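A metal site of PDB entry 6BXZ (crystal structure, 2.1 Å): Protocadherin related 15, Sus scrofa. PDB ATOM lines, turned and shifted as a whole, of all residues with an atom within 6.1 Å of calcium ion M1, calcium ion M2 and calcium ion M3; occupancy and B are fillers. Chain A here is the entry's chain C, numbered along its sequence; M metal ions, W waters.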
ATOM      1  N   GLU A  21      19.713   2.524 -29.465  1.00  0.00           N
ATOM      2  CA  GLU A  21      18.455   1.892 -29.875  1.00  0.00           C
ATOM      3  C   GLU A  21      17.694   2.740 -30.889  1.00  0.00           C
ATOM      4  O   GLU A  21      16.800   2.210 -31.551  1.00  0.00           O
ATOM      5  CB  GLU A  21      17.551   1.589 -28.679  1.00  0.00           C
ATOM      6  CG  GLU A  21      16.915   2.821 -28.037  1.00  0.00           C
ATOM      7  CD  GLU A  21      15.959   2.475 -26.897  1.00  0.00           C
ATOM      8  OE1 GLU A  21      14.913   1.826 -27.142  1.00  0.00           O
ATOM      9  OE2 GLU A  21      16.268   2.897 -25.767  1.00  0.00           O
ATOM     10  N   LEU A  22      18.011   4.032 -30.984  1.00  0.00           N
ATOM     11  CA  LEU A  22      17.449   4.910 -32.006  1.00  0.00           C
ATOM     12  C   LEU A  22      18.347   5.029 -33.250  1.00  0.00           C
ATOM     13  O   LEU A  22      18.170   5.943 -34.038  1.00  0.00           O
ATOM     14  CB  LEU A  22      17.214   6.316 -31.443  1.00  0.00           C
ATOM     15  CG  LEU A  22      16.405   6.438 -30.133  1.00  0.00           C
ATOM     16  CD1 LEU A  22      16.567   7.844 -29.545  1.00  0.00           C
ATOM     17  CD2 LEU A  22      14.937   6.125 -30.355  1.00  0.00           C
ATOM     18  N   LEU A  69      15.845  -0.839 -33.994  1.00  0.00           N
ATOM     19  CA  LEU A  69      16.240  -1.475 -32.731  1.00  0.00           C
ATOM     20  C   LEU A  69      15.343  -1.025 -31.582  1.00  0.00           C
ATOM     21  O   LEU A  69      14.637  -0.029 -31.680  1.00  0.00           O
ATOM     22  CB  LEU A  69      17.703  -1.168 -32.420  1.00  0.00           C
ATOM     23  CG  LEU A  69      18.733  -1.705 -33.426  1.00  0.00           C
ATOM     24  CD1 LEU A  69      20.113  -1.145 -33.119  1.00  0.00           C
ATOM     25  CD2 LEU A  69      18.779  -3.227 -33.468  1.00  0.00           C
ATOM     26  N   ASP A  70      15.365  -1.785 -30.503  1.00  0.00           N
ATOM     27  CA  ASP A  70      14.586  -1.463 -29.331  1.00  0.00           C
ATOM     28  C   ASP A  70      15.177  -2.129 -28.089  1.00  0.00           C
ATOM     29  O   ASP A  70      15.024  -3.329 -27.885  1.00  0.00           O
ATOM     30  CB  ASP A  70      13.128  -1.896 -29.529  1.00  0.00           C
ATOM     31  CG  ASP A  70      12.236  -1.508 -28.346  1.00  0.00           C
ATOM     32  OD1 ASP A  70      12.551  -0.577 -27.578  1.00  0.00           O
ATOM     33  OD2 ASP A  70      11.189  -2.178 -28.181  1.00  0.00           O
ATOM     34  N   TYR A  71      15.808  -1.307 -27.261  1.00  0.00           N
ATOM     35  CA  TYR A  71      16.384  -1.762 -25.985  1.00  0.00           C
ATOM     36  C   TYR A  71      15.339  -2.468 -25.114  1.00  0.00           C
ATOM     37  O   TYR A  71      15.667  -3.440 -24.442  1.00  0.00           O
ATOM     38  CB  TYR A  71      16.996  -0.576 -25.247  1.00  0.00           C
ATOM     39  CG  TYR A  71      17.689  -0.962 -23.975  1.00  0.00           C
ATOM     40  CD1 TYR A  71      16.984  -1.007 -22.764  1.00  0.00           C
ATOM     41  CD2 TYR A  71      19.044  -1.279 -23.967  1.00  0.00           C
ATOM     42  CE1 TYR A  71      17.619  -1.364 -21.583  1.00  0.00           C
ATOM     43  CE2 TYR A  71      19.693  -1.638 -22.789  1.00  0.00           C
ATOM     44  CZ  TYR A  71      18.973  -1.687 -21.612  1.00  0.00           C
ATOM     45  OH  TYR A  71      19.606  -2.039 -20.448  1.00  0.00           O
ATOM     46  N   GLU A  72      14.100  -1.983 -25.173  1.00  0.00           N
ATOM     47  CA  GLU A  72      13.013  -2.538 -24.362  1.00  0.00           C
ATOM     48  C   GLU A  72      12.494  -3.900 -24.838  1.00  0.00           C
ATOM     49  O   GLU A  72      11.770  -4.563 -24.106  1.00  0.00           O
ATOM     50  CB  GLU A  72      11.853  -1.521 -24.236  1.00  0.00           C
ATOM     51  CG  GLU A  72      12.126  -0.350 -23.296  1.00  0.00           C
ATOM     52  CD  GLU A  72      12.988   0.769 -23.859  1.00  0.00           C
ATOM     53  OE1 GLU A  72      13.855   1.343 -23.146  1.00  0.00           O
ATOM     54  OE2 GLU A  72      12.793   1.139 -25.031  1.00  0.00           O
ATOM     55  N   ASP A 110      20.491   1.916 -24.107  1.00  0.00           N
ATOM     56  CA  ASP A 110      19.185   2.473 -23.778  1.00  0.00           C
ATOM     57  C   ASP A 110      19.211   3.971 -24.089  1.00  0.00           C
ATOM     58  O   ASP A 110      20.155   4.651 -23.682  1.00  0.00           O
ATOM     59  CB  ASP A 110      18.869   2.227 -22.299  1.00  0.00           C
ATOM     60  CG  ASP A 110      17.503   2.741 -21.874  1.00  0.00           C
ATOM     61  OD1 ASP A 110      16.517   2.666 -22.654  1.00  0.00           O
ATOM     62  OD2 ASP A 110      17.414   3.194 -20.719  1.00  0.00           O
ATOM     63  N   GLU A 111      18.228   4.435 -24.857  1.00  0.00           N
ATOM     64  CA  GLU A 111      17.949   5.856 -25.004  1.00  0.00           C
ATOM     65  C   GLU A 111      16.643   6.237 -24.295  1.00  0.00           C
ATOM     66  O   GLU A 111      15.797   5.380 -24.009  1.00  0.00           O
ATOM     67  CB  GLU A 111      17.851   6.285 -26.460  1.00  0.00           C
ATOM     68  CG  GLU A 111      19.083   5.953 -27.319  1.00  0.00           C
ATOM     69  CD  GLU A 111      20.379   6.615 -26.884  1.00  0.00           C
ATOM     70  OE1 GLU A 111      20.362   7.546 -26.031  1.00  0.00           O
ATOM     71  OE2 GLU A 111      21.432   6.185 -27.406  1.00  0.00           O
ATOM     72  N   ASN A 112      16.509   7.538 -24.068  1.00  0.00           N
ATOM     73  CA  ASN A 112      15.411   8.106 -23.278  1.00  0.00           C
ATOM     74  C   ASN A 112      14.218   8.327 -24.206  1.00  0.00           C
ATOM     75  O   ASN A 112      14.009   9.432 -24.704  1.00  0.00           O
ATOM     76  CB  ASN A 112      15.842   9.420 -22.594  1.00  0.00           C
ATOM     77  CG  ASN A 112      14.899   9.856 -21.482  1.00  0.00           C
ATOM     78  OD1 ASN A 112      13.984   9.132 -21.123  1.00  0.00           O
ATOM     79  ND2 ASN A 112      15.148  11.038 -20.926  1.00  0.00           N
ATOM     80  N   ASP A 113      13.452   7.264 -24.445  1.00  0.00           N
ATOM     81  CA  ASP A 113      12.311   7.313 -25.362  1.00  0.00           C
ATOM     82  C   ASP A 113      10.969   7.031 -24.709  1.00  0.00           C
ATOM     83  O   ASP A 113       9.982   6.829 -25.404  1.00  0.00           O
ATOM     84  CB  ASP A 113      12.552   6.452 -26.639  1.00  0.00           C
ATOM     85  CG  ASP A 113      12.862   4.964 -26.363  1.00  0.00           C
ATOM     86  OD1 ASP A 113      13.082   4.540 -25.213  1.00  0.00           O
ATOM     87  OD2 ASP A 113      12.929   4.193 -27.373  1.00  0.00           O
ATOM     88  N   HIS A 114      10.899   7.056 -23.381  1.00  0.00           N
ATOM     89  CA  HIS A 114       9.630   6.920 -22.681  1.00  0.00           C
ATOM     90  C   HIS A 114       9.552   8.081 -21.703  1.00  0.00           C
ATOM     91  O   HIS A 114      10.458   8.245 -20.877  1.00  0.00           O
ATOM     92  CB  HIS A 114       9.553   5.569 -21.954  1.00  0.00           C
ATOM     93  CG  HIS A 114       9.548   4.387 -22.863  1.00  0.00           C
ATOM     94  ND1 HIS A 114       8.385   3.760 -23.275  1.00  0.00           N
ATOM     95  CD2 HIS A 114      10.571   3.701 -23.428  1.00  0.00           C
ATOM     96  CE1 HIS A 114       8.702   2.761 -24.075  1.00  0.00           C
ATOM     97  NE2 HIS A 114      10.010   2.684 -24.171  1.00  0.00           N
ATOM     98  N   PRO A 115       8.484   8.906 -21.788  1.00  0.00           N
ATOM     99  CA  PRO A 115       8.362   9.963 -20.780  1.00  0.00           C
ATOM    100  C   PRO A 115       7.843   9.403 -19.450  1.00  0.00           C
ATOM    101  O   PRO A 115       7.187   8.372 -19.447  1.00  0.00           O
ATOM    102  CB  PRO A 115       7.320  10.912 -21.411  1.00  0.00           C
ATOM    103  CG  PRO A 115       6.450  10.008 -22.207  1.00  0.00           C
ATOM    104  CD  PRO A 115       7.366   8.941 -22.761  1.00  0.00           C
ATOM    105  N   PRO A 116       8.101  10.097 -18.325  1.00  0.00           N
ATOM    106  CA  PRO A 116       7.493   9.734 -17.031  1.00  0.00           C
ATOM    107  C   PRO A 116       5.951   9.641 -17.080  1.00  0.00           C
ATOM    108  O   PRO A 116       5.305  10.477 -17.726  1.00  0.00           O
ATOM    109  CB  PRO A 116       7.938  10.875 -16.114  1.00  0.00           C
ATOM    110  CG  PRO A 116       9.202  11.384 -16.731  1.00  0.00           C
ATOM    111  CD  PRO A 116       8.952  11.304 -18.199  1.00  0.00           C
ATOM    112  N   ASP A 144       8.926   5.068 -15.726  1.00  0.00           N
ATOM    113  CA  ASP A 144       8.827   4.759 -17.152  1.00  0.00           C
ATOM    114  C   ASP A 144       9.714   3.564 -17.473  1.00  0.00           C
ATOM    115  O   ASP A 144      10.522   3.139 -16.661  1.00  0.00           O
ATOM    116  CB  ASP A 144       9.012   5.994 -18.063  1.00  0.00           C
ATOM    117  CG  ASP A 144      10.434   6.569 -18.072  1.00  0.00           C
ATOM    118  OD1 ASP A 144      11.357   5.981 -18.700  1.00  0.00           O
ATOM    119  OD2 ASP A 144      10.632   7.695 -17.550  1.00  0.00           O
ATOM    120  N   LYS A 145       9.537   3.049 -18.677  1.00  0.00           N
ATOM    121  CA  LYS A 145      10.166   1.789 -19.078  1.00  0.00           C
ATOM    122  C   LYS A 145      11.659   1.867 -19.379  1.00  0.00           C
ATOM    123  O   LYS A 145      12.281   0.821 -19.560  1.00  0.00           O
ATOM    124  CB  LYS A 145       9.437   1.179 -20.291  1.00  0.00           C
ATOM    125  CG  LYS A 145       7.918   1.178 -20.173  1.00  0.00           C
ATOM    126  CD  LYS A 145       7.236   0.092 -20.966  1.00  0.00           C
ATOM    127  CE  LYS A 145       5.730   0.262 -20.827  1.00  0.00           C
ATOM    128  NZ  LYS A 145       4.986  -0.731 -21.666  1.00  0.00           N
ATOM    129  N   ASP A 146      12.260   3.065 -19.405  1.00  0.00           N
ATOM    130  CA  ASP A 146      13.705   3.201 -19.624  1.00  0.00           C
ATOM    131  C   ASP A 146      14.456   2.726 -18.400  1.00  0.00           C
ATOM    132  O   ASP A 146      13.870   2.507 -17.351  1.00  0.00           O
ATOM    133  CB  ASP A 146      14.073   4.657 -19.942  1.00  0.00           C
ATOM    134  CG  ASP A 146      13.432   5.176 -21.227  1.00  0.00           C
ATOM    135  OD1 ASP A 146      13.428   4.432 -22.208  1.00  0.00           O
ATOM    136  OD2 ASP A 146      12.938   6.323 -21.277  1.00  0.00           O
ATOM    137  N   THR A 147      15.776   2.606 -18.520  1.00  0.00           N
ATOM    138  CA  THR A 147      16.629   2.100 -17.459  1.00  0.00           C
ATOM    139  C   THR A 147      17.474   3.208 -16.850  1.00  0.00           C
ATOM    140  O   THR A 147      17.729   4.248 -17.494  1.00  0.00           O
ATOM    141  CB  THR A 147      17.586   1.027 -18.021  1.00  0.00           C
ATOM    142  OG1 THR A 147      16.829   0.009 -18.689  1.00  0.00           O
ATOM    143  CG2 THR A 147      18.458   0.393 -16.926  1.00  0.00           C
ATOM    144  N   TYR A 150      17.611   7.317 -17.152  1.00  0.00           N
ATOM    145  CA  TYR A 150      16.511   7.661 -18.061  1.00  0.00           C
ATOM    146  C   TYR A 150      15.078   7.378 -17.573  1.00  0.00           C
ATOM    147  O   TYR A 150      14.096   7.733 -18.264  1.00  0.00           O
ATOM    148  CB  TYR A 150      16.763   7.052 -19.460  1.00  0.00           C
ATOM    149  CG  TYR A 150      17.963   7.634 -20.194  1.00  0.00           C
ATOM    150  CD1 TYR A 150      18.396   8.955 -19.977  1.00  0.00           C
ATOM    151  CD2 TYR A 150      18.661   6.868 -21.139  1.00  0.00           C
ATOM    152  CE1 TYR A 150      19.474   9.478 -20.663  1.00  0.00           C
ATOM    153  CE2 TYR A 150      19.747   7.402 -21.823  1.00  0.00           C
ATOM    154  CZ  TYR A 150      20.146   8.703 -21.582  1.00  0.00           C
ATOM    155  OH  TYR A 150      21.193   9.256 -22.225  1.00  0.00           O
ATOM    156  N   SER A 151      14.956   6.745 -16.392  1.00  0.00           N
ATOM    157  CA  SER A 151      13.690   6.715 -15.673  1.00  0.00           C
ATOM    158  C   SER A 151      13.838   7.143 -14.190  1.00  0.00           C
ATOM    159  O   SER A 151      13.005   6.793 -13.379  1.00  0.00           O
ATOM    160  CB  SER A 151      13.085   5.319 -15.753  1.00  0.00           C
ATOM    161  OG  SER A 151      13.942   4.393 -15.116  1.00  0.00           O
ATOM    162  N   MET A 153      13.697  10.015 -11.506  1.00  0.00           N
ATOM    163  CA  MET A 153      12.850  11.202 -11.531  1.00  0.00           C
ATOM    164  C   MET A 153      13.334  12.332 -10.635  1.00  0.00           C
ATOM    165  O   MET A 153      13.794  12.081  -9.532  1.00  0.00           O
ATOM    166  CB  MET A 153      11.438  10.804 -11.079  1.00  0.00           C
ATOM    167  CG  MET A 153      10.797   9.717 -11.921  1.00  0.00           C
ATOM    168  SD  MET A 153      10.701  10.154 -13.664  1.00  0.00           S
ATOM    169  CE  MET A 153      10.212   8.591 -14.403  1.00  0.00           C
ATOM    170  N   ASP A 200      12.545  12.946 -15.977  1.00  0.00           N
ATOM    171  CA  ASP A 200      13.558  11.888 -15.860  1.00  0.00           C
ATOM    172  C   ASP A 200      14.956  12.448 -16.163  1.00  0.00           C
ATOM    173  O   ASP A 200      15.129  13.633 -16.476  1.00  0.00           O
ATOM    174  CB  ASP A 200      13.201  10.669 -16.720  1.00  0.00           C
ATOM    175  CG  ASP A 200      13.072  10.996 -18.189  1.00  0.00           C
ATOM    176  OD1 ASP A 200      13.760  11.913 -18.687  1.00  0.00           O
ATOM    177  OD2 ASP A 200      12.235  10.355 -18.851  1.00  0.00           O
ATOM    178  N   LEU A 206      12.792  13.962 -20.177  1.00  0.00           N
ATOM    179  CA  LEU A 206      11.389  14.081 -20.554  1.00  0.00           C
ATOM    180  C   LEU A 206      10.515  14.244 -19.307  1.00  0.00           C
ATOM    181  O   LEU A 206      10.912  13.863 -18.213  1.00  0.00           O
ATOM    182  CB  LEU A 206      10.943  12.845 -21.336  1.00  0.00           C
ATOM    183  CG  LEU A 206      11.707  12.482 -22.630  1.00  0.00           C
ATOM    184  CD1 LEU A 206      11.224  11.154 -23.200  1.00  0.00           C
ATOM    185  CD2 LEU A 206      11.579  13.582 -23.665  1.00  0.00           C
HETATM  186 CA    CA M   1      12.364   8.152 -19.663  1.00  0.00          CA
HETATM  187 CA    CA M   2      14.727   3.343 -23.863  1.00  0.00          CA
HETATM  188 CA    CA M   3      12.577   1.773 -27.298  1.00  0.00          CA
HETATM  189  O   HOH W   1      12.876   2.010 -29.742  1.00  0.00           O
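A ring nitrogen (NE2) of His 114 lies close to the side-chain carboxylate (OE2) of Glu 72, at 3.3 Å.
The side-chain carboxylate of Asp 110 is in hydrogen-bond range of the backbone NH of Thr 147 (2.8 Å).
OE1 of Glu 21 lies close to N of Tyr 71 (3.3 Å).
OD1 of Asp 200 lies within hydrogen-bond range of N of Leu 206, 2.7 Å away.
O of Asp 146 sits at hydrogen-bond distance from OG of Ser 151, at 2.9 Å.
Within 4 Å of calcium ion M1: Asn 112, His 114, Asp 144, Asp 146, Tyr 150 and Asp 200.
Along chain A the residues within 4 Å of calcium ion M1 span positions 112 to 200.
The nearest printed residue that does not touch calcium ion M1 is Ser 151 (4.4 Å).
Within 4 Å of calcium ion M2: Glu 21, Glu 72, Asp 110, Glu 111, Asp 113 and Asp 146.
Of the 22 residues printed, 4 come within 4 Å of calcium ion M3.
The nearest printed residue that does not touch calcium ion M3 is His 114 (4.1 Å).
Calcium ion M1 is bound by O of His 114, O of Tyr 150, OD2 of Asp 200, OD1 of Asn 112, OD2 of Asp 146, OD1 of Asp 144 and OD2 of Asp 144.
Calcium ion M1 has seven donor atoms within binding distance.
Calcium ion M2 is bound by the side-chain carboxylate (OD1) of Asp 110 (2.3 Å), the side-chain carboxylate (OE1) of Glu 72 (2.3 Å), the backbone carbonyl oxygen (O) of Glu 111 (2.3 Å), the side-chain carboxylate (OD1) of Asp 146 (2.4 Å), the side-chain carboxylate (OD1) of Asp 113 (2.4 Å) and the side-chain carboxylate (OE2) of Glu 21 (2.5 Å).
Calcium ion M3 is bound by OE1 of Glu 21 (2.3 Å), OE2 of Glu 72 (2.4 Å), OD1 of Asp 70 (2.4 Å), OD2 of Asp 113 (2.4 Å) and water W1 (2.5 Å).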
